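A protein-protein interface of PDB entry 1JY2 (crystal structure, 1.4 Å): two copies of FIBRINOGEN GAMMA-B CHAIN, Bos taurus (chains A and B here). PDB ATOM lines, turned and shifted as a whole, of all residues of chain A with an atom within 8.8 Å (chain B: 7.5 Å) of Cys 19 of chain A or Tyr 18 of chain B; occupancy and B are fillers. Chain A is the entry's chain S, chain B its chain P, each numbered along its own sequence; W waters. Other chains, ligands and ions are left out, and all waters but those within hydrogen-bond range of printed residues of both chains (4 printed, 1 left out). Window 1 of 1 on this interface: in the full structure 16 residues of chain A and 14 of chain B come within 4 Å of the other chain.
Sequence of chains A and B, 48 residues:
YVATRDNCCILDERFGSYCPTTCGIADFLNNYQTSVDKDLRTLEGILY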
ATOM      1  N   VAL A   2      28.772  20.647  30.368  1.00  0.00           N
ATOM      2  CA  VAL A   2      30.050  21.141  29.765  1.00  0.00           C
ATOM      3  C   VAL A   2      30.698  20.061  28.901  1.00  0.00           C
ATOM      4  O   VAL A   2      30.780  18.898  29.304  1.00  0.00           O
ATOM      5  CB  VAL A   2      31.057  21.578  30.863  1.00  0.00           C
ATOM      6  CG1 VAL A   2      31.413  20.397  31.750  1.00  0.00           C
ATOM      7  CG2 VAL A   2      32.313  22.142  30.225  1.00  0.00           C
ATOM      8  N   ALA A   3      31.155  20.449  27.709  1.00  0.00           N
ATOM      9  CA  ALA A   3      31.789  19.502  26.801  1.00  0.00           C
ATOM     10  C   ALA A   3      33.142  19.026  27.351  1.00  0.00           C
ATOM     11  O   ALA A   3      33.929  19.831  27.852  1.00  0.00           O
ATOM     12  CB  ALA A   3      31.974  20.154  25.411  1.00  0.00           C
ATOM     13  N   ASN A   7      32.444  13.112  26.762  1.00  0.00           N
ATOM     14  CA  ASN A   7      31.049  13.272  26.363  1.00  0.00           C
ATOM     15  C   ASN A   7      30.848  14.052  25.053  1.00  0.00           C
ATOM     16  O   ASN A   7      29.714  14.266  24.617  1.00  0.00           O
ATOM     17  CB  ASN A   7      30.258  13.952  27.489  1.00  0.00           C
ATOM     18  CG  ASN A   7      30.670  15.401  27.708  1.00  0.00           C
ATOM     19  OD1 ASN A   7      31.226  16.055  26.815  1.00  0.00           O
ATOM     20  ND2 ASN A   7      30.373  15.921  28.894  1.00  0.00           N
ATOM     21  N   CYS A   8      31.945  14.434  24.411  1.00  0.00           N
ATOM     22  CA  CYS A   8      31.869  15.227  23.186  1.00  0.00           C
ATOM     23  C   CYS A   8      33.035  14.857  22.274  1.00  0.00           C
ATOM     24  O   CYS A   8      34.138  15.391  22.428  1.00  0.00           O
ATOM     25  CB  CYS A   8      31.971  16.674  23.601  1.00  0.00           C
ATOM     26  SG  CYS A   8      31.556  17.870  22.290  1.00  0.00           S
ATOM     27  N   CYS A   9      32.775  14.013  21.286  1.00  0.00           N
ATOM     28  CA  CYS A   9      33.858  13.526  20.438  1.00  0.00           C
ATOM     29  C   CYS A   9      34.515  14.507  19.481  1.00  0.00           C
ATOM     30  O   CYS A   9      35.620  14.249  18.995  1.00  0.00           O
ATOM     31  CB  CYS A   9      33.411  12.257  19.695  1.00  0.00           C
ATOM     32  SG  CYS A   9      32.761  12.447  17.998  1.00  0.00           S
ATOM     33  N   ILE A  10      33.865  15.639  19.224  1.00  0.00           N
ATOM     34  CA  ILE A  10      34.446  16.640  18.328  1.00  0.00           C
ATOM     35  C   ILE A  10      35.072  17.774  19.117  1.00  0.00           C
ATOM     36  O   ILE A  10      35.611  18.715  18.520  1.00  0.00           O
ATOM     37  CB  ILE A  10      33.392  17.291  17.400  1.00  0.00           C
ATOM     38  CG1 ILE A  10      32.237  17.846  18.246  1.00  0.00           C
ATOM     39  CG2 ILE A  10      32.925  16.296  16.347  1.00  0.00           C
ATOM     40  CD1 ILE A  10      31.305  18.787  17.456  1.00  0.00           C
ATOM     41  N   LEU A  11      35.022  17.698  20.446  1.00  0.00           N
ATOM     42  CA  LEU A  11      35.546  18.785  21.258  1.00  0.00           C
ATOM     43  C   LEU A  11      36.940  19.286  20.894  1.00  0.00           C
ATOM     44  O   LEU A  11      37.900  18.511  20.837  1.00  0.00           O
ATOM     45  CB  LEU A  11      35.535  18.440  22.757  1.00  0.00           C
ATOM     46  CG  LEU A  11      36.135  19.494  23.689  1.00  0.00           C
ATOM     47  CD1 LEU A  11      35.393  20.829  23.547  1.00  0.00           C
ATOM     48  CD2 LEU A  11      36.049  18.995  25.123  1.00  0.00           C
ATOM     49  N   PHE A  15      37.980  26.384  20.329  1.00  0.00           N
ATOM     50  CA  PHE A  15      36.761  27.004  19.798  1.00  0.00           C
ATOM     51  C   PHE A  15      35.750  27.506  20.836  1.00  0.00           C
ATOM     52  O   PHE A  15      34.633  27.918  20.484  1.00  0.00           O
ATOM     53  CB  PHE A  15      36.098  26.059  18.782  1.00  0.00           C
ATOM     54  CG  PHE A  15      36.891  25.878  17.539  1.00  0.00           C
ATOM     55  CD1 PHE A  15      37.938  24.942  17.485  1.00  0.00           C
ATOM     56  CD2 PHE A  15      36.625  26.662  16.399  1.00  0.00           C
ATOM     57  CE1 PHE A  15      38.695  24.788  16.324  1.00  0.00           C
ATOM     58  CE2 PHE A  15      37.372  26.518  15.235  1.00  0.00           C
ATOM     59  CZ  PHE A  15      38.414  25.578  15.189  1.00  0.00           C
ATOM     60  N   GLY A  16      36.127  27.480  22.116  1.00  0.00           N
ATOM     61  CA  GLY A  16      35.237  28.007  23.135  1.00  0.00           C
ATOM     62  C   GLY A  16      34.213  27.020  23.659  1.00  0.00           C
ATOM     63  O   GLY A  16      34.259  25.835  23.310  1.00  0.00           O
ATOM     64  N   SER A  17      33.285  27.517  24.475  1.00  0.00           N
ATOM     65  CA  SER A  17      32.242  26.688  25.082  1.00  0.00           C
ATOM     66  C   SER A  17      31.201  26.259  24.061  1.00  0.00           C
ATOM     67  O   SER A  17      30.939  26.978  23.090  1.00  0.00           O
ATOM     68  CB  SER A  17      31.568  27.448  26.223  1.00  0.00           C
ATOM     69  OG  SER A  17      32.507  27.757  27.239  1.00  0.00           O
ATOM     70  N   TYR A  18      30.628  25.083  24.270  1.00  0.00           N
ATOM     71  CA  TYR A  18      29.641  24.503  23.355  1.00  0.00           C
ATOM     72  C   TYR A  18      28.219  24.732  23.826  1.00  0.00           C
ATOM     73  O   TYR A  18      27.938  24.824  25.027  1.00  0.00           O
ATOM     74  CB  TYR A  18      29.933  22.995  23.185  1.00  0.00           C
ATOM     75  CG  TYR A  18      31.120  22.701  22.284  1.00  0.00           C
ATOM     76  CD1 TYR A  18      32.231  23.542  22.226  1.00  0.00           C
ATOM     77  CD2 TYR A  18      31.135  21.549  21.499  1.00  0.00           C
ATOM     78  CE1 TYR A  18      33.350  23.239  21.392  1.00  0.00           C
ATOM     79  CE2 TYR A  18      32.239  21.235  20.671  1.00  0.00           C
ATOM     80  CZ  TYR A  18      33.341  22.083  20.623  1.00  0.00           C
ATOM     81  OH  TYR A  18      34.407  21.756  19.811  1.00  0.00           O
ATOM     82  N   CYS A  19      27.317  24.784  22.845  1.00  0.00           N
ATOM     83  CA  CYS A  19      25.899  25.047  23.037  1.00  0.00           C
ATOM     84  C   CYS A  19      25.065  24.246  22.074  1.00  0.00           C
ATOM     85  O   CYS A  19      25.565  23.763  21.074  1.00  0.00           O
ATOM     86  CB  CYS A  19      25.591  26.548  22.637  1.00  0.00           C
ATOM     87  SG  CYS A  19      26.403  27.781  23.678  1.00  0.00           S
ATOM     88  N   PRO A  20      23.768  24.114  22.342  1.00  0.00           N
ATOM     89  CA  PRO A  20      22.931  23.395  21.375  1.00  0.00           C
ATOM     90  C   PRO A  20      22.918  24.234  20.069  1.00  0.00           C
ATOM     91  O   PRO A  20      23.267  25.447  20.089  1.00  0.00           O
ATOM     92  CB  PRO A  20      21.530  23.443  21.978  1.00  0.00           C
ATOM     93  CG  PRO A  20      21.741  23.709  23.414  1.00  0.00           C
ATOM     94  CD  PRO A  20      23.005  24.523  23.537  1.00  0.00           C
ATOM     95  N   THR A  21      22.535  23.632  18.956  1.00  0.00           N
ATOM     96  CA  THR A  21      22.408  24.404  17.717  1.00  0.00           C
ATOM     97  C   THR A  21      20.958  24.926  17.645  1.00  0.00           C
ATOM     98  O   THR A  21      20.086  24.489  18.390  1.00  0.00           O
ATOM     99  CB  THR A  21      22.611  23.545  16.480  1.00  0.00           C
ATOM    100  OG1 THR A  21      21.506  22.647  16.357  1.00  0.00           O
ATOM    101  CG2 THR A  21      23.907  22.773  16.580  1.00  0.00           C
ATOM    102  N   THR A  22      20.710  25.884  16.742  1.00  0.00           N
ATOM    103  CA  THR A  22      19.343  26.361  16.634  1.00  0.00           C
ATOM    104  C   THR A  22      18.401  25.312  16.043  1.00  0.00           C
ATOM    105  O   THR A  22      17.191  25.462  16.122  1.00  0.00           O
ATOM    106  CB  THR A  22      19.277  27.657  15.821  1.00  0.00           C
ATOM    107  OG1 THR A  22      19.939  27.471  14.573  1.00  0.00           O
ATOM    108  CG2 THR A  22      19.902  28.805  16.577  1.00  0.00           C
ATOM    109  N   CYS A  23      18.952  24.254  15.422  1.00  0.00           N
ATOM    110  CA  CYS A  23      18.067  23.147  15.003  1.00  0.00           C
ATOM    111  C   CYS A  23      17.603  22.411  16.272  1.00  0.00           C
ATOM    112  O   CYS A  23      16.440  22.025  16.395  1.00  0.00           O
ATOM    113  CB  CYS A  23      18.775  22.133  14.117  1.00  0.00           C
ATOM    114  SG  CYS A  23      19.194  22.681  12.448  1.00  0.00           S
ATOM    115  N   GLY A  24      18.513  22.237  17.239  1.00  0.00           N
ATOM    116  CA  GLY A  24      18.125  21.608  18.494  1.00  0.00           C
ATOM    117  C   GLY A  24      17.063  22.442  19.194  1.00  0.00           C
ATOM    118  O   GLY A  24      16.119  21.911  19.774  1.00  0.00           O
ATOM    119  N   ILE A  25      17.252  23.763  19.139  1.00  0.00           N
ATOM    120  CA  ILE A  25      16.282  24.688  19.726  1.00  0.00           C
ATOM    121  C   ILE A  25      14.922  24.560  19.006  1.00  0.00           C
ATOM    122  O   ILE A  25      13.899  24.455  19.661  1.00  0.00           O
ATOM    123  CB  ILE A  25      16.786  26.174  19.592  1.00  0.00           C
ATOM    124  CG1 ILE A  25      18.077  26.390  20.401  1.00  0.00           C
ATOM    125  CG2 ILE A  25      15.682  27.154  20.062  1.00  0.00           C
ATOM    126  CD1 ILE A  25      17.960  26.076  21.893  1.00  0.00           C
ATOM    127  N   ASP B   6      28.379  14.289  13.600  1.00  0.00           N
ATOM    128  CA  ASP B   6      27.675  15.497  14.021  1.00  0.00           C
ATOM    129  C   ASP B   6      26.619  15.163  15.075  1.00  0.00           C
ATOM    130  O   ASP B   6      25.713  15.948  15.333  1.00  0.00           O
ATOM    131  CB  ASP B   6      27.041  16.162  12.802  1.00  0.00           C
ATOM    132  CG  ASP B   6      26.173  15.216  12.026  1.00  0.00           C
ATOM    133  OD1 ASP B   6      25.843  15.529  10.860  1.00  0.00           O
ATOM    134  OD2 ASP B   6      25.812  14.154  12.588  1.00  0.00           O
ATOM    135  N   ASN B   7      26.745  14.003  15.720  1.00  0.00           N
ATOM    136  CA  ASN B   7      25.761  13.612  16.733  1.00  0.00           C
ATOM    137  C   ASN B   7      26.452  12.970  17.929  1.00  0.00           C
ATOM    138  O   ASN B   7      25.849  12.150  18.647  1.00  0.00           O
ATOM    139  CB  ASN B   7      24.761  12.616  16.129  1.00  0.00           C
ATOM    140  CG  ASN B   7      25.452  11.362  15.603  1.00  0.00           C
ATOM    141  OD1 ASN B   7      26.684  11.251  15.678  1.00  0.00           O
ATOM    142  ND2 ASN B   7      24.675  10.418  15.081  1.00  0.00           N
ATOM    143  N   CYS B   8      27.688  13.368  18.174  1.00  0.00           N
ATOM    144  CA  CYS B   8      28.486  12.774  19.244  1.00  0.00           C
ATOM    145  C   CYS B   8      28.779  13.723  20.408  1.00  0.00           C
ATOM    146  O   CYS B   8      29.747  13.546  21.169  1.00  0.00           O
ATOM    147  CB  CYS B   8      29.799  12.260  18.616  1.00  0.00           C
ATOM    148  SG  CYS B   8      31.061  13.550  18.256  1.00  0.00           S
ATOM    149  N   CYS B   9      27.933  14.745  20.573  1.00  0.00           N
ATOM    150  CA  CYS B   9      28.150  15.700  21.657  1.00  0.00           C
ATOM    151  C   CYS B   9      26.817  16.116  22.268  1.00  0.00           C
ATOM    152  O   CYS B   9      26.572  17.295  22.532  1.00  0.00           O
ATOM    153  CB  CYS B   9      28.886  16.939  21.123  1.00  0.00           C
ATOM    154  SG  CYS B   9      29.515  18.087  22.368  1.00  0.00           S
ATOM    155  N   ILE B  10      25.954  15.133  22.523  1.00  0.00           N
ATOM    156  CA  ILE B  10      24.634  15.411  23.094  1.00  0.00           C
ATOM    157  C   ILE B  10      24.737  15.582  24.602  1.00  0.00           C
ATOM    158  O   ILE B  10      24.720  14.601  25.355  1.00  0.00           O
ATOM    159  CB  ILE B  10      23.646  14.274  22.760  1.00  0.00           C
ATOM    160  CG1 ILE B  10      23.657  14.026  21.251  1.00  0.00           C
ATOM    161  CG2 ILE B  10      22.233  14.614  23.287  1.00  0.00           C
ATOM    162  CD1 ILE B  10      22.830  12.812  20.766  1.00  0.00           C
ATOM    163  N   LEU B  11      24.838  16.835  25.040  1.00  0.00           N
ATOM    164  CA  LEU B  11      24.998  17.171  26.451  1.00  0.00           C
ATOM    165  C   LEU B  11      23.678  17.320  27.217  1.00  0.00           C
ATOM    166  O   LEU B  11      23.675  17.395  28.453  1.00  0.00           O
ATOM    167  CB  LEU B  11      25.859  18.440  26.595  1.00  0.00           C
ATOM    168  CG  LEU B  11      27.197  18.426  25.837  1.00  0.00           C
ATOM    169  CD1 LEU B  11      28.041  19.606  26.270  1.00  0.00           C
ATOM    170  CD2 LEU B  11      27.972  17.127  26.133  1.00  0.00           C
ATOM    171  N   ASP B  12      22.572  17.364  26.477  1.00  0.00           N
ATOM    172  CA  ASP B  12      21.213  17.451  27.026  1.00  0.00           C
ATOM    173  C   ASP B  12      20.345  16.848  25.923  1.00  0.00           C
ATOM    174  O   ASP B  12      20.230  17.414  24.823  1.00  0.00           O
ATOM    175  CB  ASP B  12      20.803  18.906  27.313  1.00  0.00           C
ATOM    176  CG  ASP B  12      19.449  19.005  28.028  1.00  0.00           C
ATOM    177  OD1 ASP B  12      18.543  18.218  27.700  1.00  0.00           O
ATOM    178  OD2 ASP B  12      19.294  19.889  28.898  1.00  0.00           O
ATOM    179  N   GLU B  13      19.774  15.661  26.188  1.00  0.00           N
ATOM    180  CA  GLU B  13      18.950  14.961  25.217  1.00  0.00           C
ATOM    181  C   GLU B  13      17.787  15.780  24.657  1.00  0.00           C
ATOM    182  O   GLU B  13      17.327  15.539  23.533  1.00  0.00           O
ATOM    183  CB  GLU B  13      18.424  13.657  25.841  1.00  0.00           C
ATOM    184  CG  GLU B  13      19.544  12.715  26.292  1.00  0.00           C
ATOM    185  CD  GLU B  13      19.038  11.522  27.103  1.00  0.00           C
ATOM    186  OE1 GLU B  13      18.172  10.775  26.590  1.00  0.00           O
ATOM    187  OE2 GLU B  13      19.506  11.325  28.252  1.00  0.00           O
ATOM    188  N   ARG B  14      17.314  16.761  25.421  1.00  0.00           N
ATOM    189  CA  ARG B  14      16.213  17.579  24.936  1.00  0.00           C
ATOM    190  C   ARG B  14      16.637  18.508  23.819  1.00  0.00           C
ATOM    191  O   ARG B  14      15.804  18.887  22.991  1.00  0.00           O
ATOM    192  CB  ARG B  14      15.645  18.467  26.043  1.00  0.00           C
ATOM    193  CG  ARG B  14      14.994  17.688  27.170  1.00  0.00           C
ATOM    194  CD  ARG B  14      14.654  18.619  28.305  1.00  0.00           C
ATOM    195  NE  ARG B  14      15.841  19.237  28.880  1.00  0.00           N
ATOM    196  CZ  ARG B  14      15.811  20.109  29.878  1.00  0.00           C
ATOM    197  NH1 ARG B  14      14.631  20.463  30.405  1.00  0.00           N
ATOM    198  NH2 ARG B  14      16.936  20.620  30.359  1.00  0.00           N
ATOM    199  N   PHE B  15      17.924  18.850  23.796  1.00  0.00           N
ATOM    200  CA  PHE B  15      18.404  19.832  22.829  1.00  0.00           C
ATOM    201  C   PHE B  15      19.337  19.405  21.722  1.00  0.00           C
ATOM    202  O   PHE B  15      19.857  20.232  21.004  1.00  0.00           O
ATOM    203  CB  PHE B  15      19.030  21.006  23.597  1.00  0.00           C
ATOM    204  CG  PHE B  15      18.035  21.773  24.422  1.00  0.00           C
ATOM    205  CD1 PHE B  15      17.877  21.523  25.779  1.00  0.00           C
ATOM    206  CD2 PHE B  15      17.184  22.695  23.806  1.00  0.00           C
ATOM    207  CE1 PHE B  15      16.874  22.179  26.520  1.00  0.00           C
ATOM    208  CE2 PHE B  15      16.177  23.359  24.535  1.00  0.00           C
ATOM    209  CZ  PHE B  15      16.025  23.097  25.886  1.00  0.00           C
ATOM    210  N   GLY B  16      19.563  18.106  21.564  1.00  0.00           N
ATOM    211  CA  GLY B  16      20.440  17.676  20.494  1.00  0.00           C
ATOM    212  C   GLY B  16      21.935  17.728  20.750  1.00  0.00           C
ATOM    213  O   GLY B  16      22.394  17.942  21.867  1.00  0.00           O
ATOM    214  N   SER B  17      22.703  17.543  19.682  1.00  0.00           N
ATOM    215  CA  SER B  17      24.160  17.553  19.812  1.00  0.00           C
ATOM    216  C   SER B  17      24.718  18.988  19.816  1.00  0.00           C
ATOM    217  O   SER B  17      24.260  19.835  19.039  1.00  0.00           O
ATOM    218  CB  SER B  17      24.782  16.688  18.689  1.00  0.00           C
ATOM    219  OG  SER B  17      26.141  16.384  18.948  1.00  0.00           O
ATOM    220  N   TYR B  18      25.701  19.248  20.670  1.00  0.00           N
ATOM    221  CA  TYR B  18      26.260  20.600  20.847  1.00  0.00           C
ATOM    222  C   TYR B  18      27.425  20.948  19.935  1.00  0.00           C
ATOM    223  O   TYR B  18      28.161  20.076  19.445  1.00  0.00           O
ATOM    224  CB  TYR B  18      26.687  20.773  22.298  1.00  0.00           C
ATOM    225  CG  TYR B  18      25.544  20.896  23.287  1.00  0.00           C
ATOM    226  CD1 TYR B  18      24.357  20.180  23.120  1.00  0.00           C
ATOM    227  CD2 TYR B  18      25.664  21.731  24.397  1.00  0.00           C
ATOM    228  CE1 TYR B  18      23.319  20.288  24.044  1.00  0.00           C
ATOM    229  CE2 TYR B  18      24.622  21.856  25.326  1.00  0.00           C
ATOM    230  CZ  TYR B  18      23.462  21.123  25.131  1.00  0.00           C
ATOM    231  OH  TYR B  18      22.416  21.250  26.012  1.00  0.00           O
ATOM    232  N   CYS B  19      27.613  22.253  19.761  1.00  0.00           N
ATOM    233  CA  CYS B  19      28.626  22.824  18.889  1.00  0.00           C
ATOM    234  C   CYS B  19      29.155  24.095  19.486  1.00  0.00           C
ATOM    235  O   CYS B  19      28.531  24.697  20.366  1.00  0.00           O
ATOM    236  CB  CYS B  19      27.965  23.238  17.541  1.00  0.00           C
ATOM    237  SG  CYS B  19      27.241  21.860  16.604  1.00  0.00           S
ATOM    238  N   PRO B  20      30.303  24.539  18.980  1.00  0.00           N
ATOM    239  CA  PRO B  20      30.821  25.799  19.481  1.00  0.00           C
ATOM    240  C   PRO B  20      29.880  26.868  18.837  1.00  0.00           C
ATOM    241  O   PRO B  20      29.098  26.611  17.865  1.00  0.00           O
ATOM    242  CB  PRO B  20      32.232  25.876  18.902  1.00  0.00           C
ATOM    243  CG  PRO B  20      32.196  24.992  17.717  1.00  0.00           C
ATOM    244  CD  PRO B  20      31.243  23.873  18.066  1.00  0.00           C
ATOM    245  N   THR B  21      29.911  28.045  19.421  1.00  0.00           N
ATOM    246  CA  THR B  21      29.132  29.164  18.893  1.00  0.00           C
ATOM    247  C   THR B  21      29.923  29.855  17.771  1.00  0.00           C
ATOM    248  O   THR B  21      31.137  29.680  17.618  1.00  0.00           O
ATOM    249  CB  THR B  21      28.881  30.250  19.960  1.00  0.00           C
ATOM    250  OG1 THR B  21      30.122  30.891  20.275  1.00  0.00           O
ATOM    251  CG2 THR B  21      28.278  29.625  21.241  1.00  0.00           C
HETATM  252  O   HOH W   1      15.967  19.220  20.210  1.00  0.00           O
HETATM  253  O   HOH W   2      32.164  28.521  21.359  1.00  0.00           O
HETATM  254  O   HOH W   3      27.488  12.950  25.283  1.00  0.00           O
HETATM  255  O   HOH W   4      21.714  20.833  19.092  1.00  0.00           O
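Along chain B the printed residues that touch a printed residue of chain A span positions 8 to 21.
Among the printed residues, no Asp or Glu carboxylate lies within 4 Å of a Lys or Arg side-chain nitrogen of the other chain.
N of Cys 8 of chain B lies within hydrogen-bond range of OG of Ser 17 of chain B.
OG of Ser 17 of chain B sits at hydrogen-bond distance from N of Cys 9 of chain B.
The backbone NH of Cys 23 of chain A lies close to the side-chain hydroxyl of Thr 21 of chain A.
O of Val 2 of chain A is in hydrogen-bond range of ND2 of Asn 7 of chain A, 3.0 Å away.
OG1 of Thr 21 of chain A lies within hydrogen-bond range of N of Gly 24 of chain A, at 3.1 Å.
The backbone carbonyl oxygen (O) of Cys 9 of chain B lies within hydrogen-bond range of the backbone NH (N) of Tyr 18 of chain B (2.8 Å).
Of the printed residues of chain B, Val 2 of chain A touches Leu 11 (3.8 Å).
Printed residues of chain B within 4 Å of Asn 7 of chain A: Cys 8 (3.5 Å), Cys 9 (3.6 Å) and Leu 11 (3.5 Å).
Of the printed residues of chain B, Phe 15 of chain A touches Pro 20.
Cys 19 of chain A touches three residues of chain B.
Cys 23 of chain A touches none of the printed residues of chain B.
Of the printed residues of chain A, Cys 9 of chain B touches Asn 7, Cys 8 and Tyr 18.
Ile 10 of chain B touches none of the printed residues of chain A.
Printed residues of chain A within 4 Å of Phe 15 of chain B: Pro 20 (3.7 Å), Gly 24 (3.3 Å) and Ile 25 (3.96 Å).
Ser 17 of chain B touches just one residue of chain A: Thr 21.
Printed residues of chain A within 4 Å of Tyr 18 of chain B: Ile 10 (3.9 Å), Tyr 18 (3.9 Å), Cys 19 (3.2 Å) and Pro 20 (3.5 Å).
The nearest residue of chain B that does not touch Cys 19 of chain A is Ser 17 of chain B (4.6 Å).
The nearest residue of chain A that does not touch Tyr 18 of chain B is Cys 8 of chain A (4.9 Å).
The nearest printed residue of chain B that does not touch Phe 15 of chain A is Thr 21 of chain B (4.8 Å).
The backbone carbonyl oxygen of Cys 19 of chain B sits at hydrogen-bond distance from the backbone NH of Cys 19 of chain A (2.8 Å).
The side-chain sulfur (SG) of Cys 8 of chain B is disulfide-bonded to the side-chain sulfur (SG) of Cys 9 of chain A, 2.0 Å away.
The side-chain sulfur of Cys 9 of chain B is disulfide-bonded to the side-chain sulfur of Cys 8 of chain A (2.1 Å).
The backbone NH (N) of Ile 10 of chain A lies within hydrogen-bond range of the side-chain sulfur (SG) of Cys 8 of chain B, at 3.6 Å.
Among the printed residues, merely in contact across the chains: Val 2 of chain A with Leu 11 of chain B, Ala 3 of chain A with Leu 11 of chain B, Asn 7 of chain A with Cys 8 of chain B, Asn 7 of chain A with Cys 9 of chain B, Asn 7 of chain A with Leu 11 of chain B, Cys 8 of chain A with Cys 8 of chain B, Ile 10 of chain A with Tyr 18 of chain B, Phe 15 of chain A with Pro 20 of chain B, Ser 17 of chain A with Pro 20 of chain B, Ser 17 of chain A with Thr 21 of chain B, Tyr 18 of chain A with Cys 9 of chain B, Tyr 18 of chain A with Tyr 18 of chain B, Tyr 18 of chain A with Cys 19 of chain B, Tyr 18 of chain A with Pro 20 of chain B, Cys 19 of chain A with Tyr 18 of chain B, Cys 19 of chain A with Thr 21 of chain B, Pro 20 of chain A with Phe 15 of chain B, Pro 20 of chain A with Tyr 18 of chain B, Thr 21 of chain A with Ser 17 of chain B, Thr 21 of chain A with Cys 19 of chain B, Gly 24 of chain A with Phe 15 of chain B and Ile 25 of chain A with Phe 15 of chain B.
Water W2 lies within hydrogen-bond range of O of Ser 17 of chain A, O of Phe 15 of chain A and N of Thr 21 of chain B.
Water W3 bridges the backbone carbonyl oxygen of Asn 7 of chain A (2.7 Å) and the backbone carbonyl oxygen of Ile 10 of chain B (3.2 Å).
Water W1 lies within hydrogen-bond range of O of Gly 24 of chain A and O of Arg 14 of chain B.
Water W4 lies within hydrogen-bond range of O of Phe 15 of chain B (2.7 Å), O of Ser 17 of chain B (2.7 Å) and N of Thr 21 of chain A (2.9 Å).
Asn 7 of chain A touches Cys 9 of chain B, but with the chains exchanged Cys 9 of chain A does not touch Asn 7 of chain B (6.3 Å).
Asn 7 of chain A touches Leu 11 of chain B, but with the chains exchanged Leu 11 of chain A does not touch Asn 7 of chain B (10.1 Å).
Cys 8 of chain A touches its own counterpart, Cys 8 of chain B.
Ile 10 of chain A touches Tyr 18 of chain B, but with the chains exchanged Tyr 18 of chain A does not touch Ile 10 of chain B (8.3 Å).
Positions printed for both chains: 7, 8, 9, 10, 11, 15, 16, 17, 18, 19, 20 and 21.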
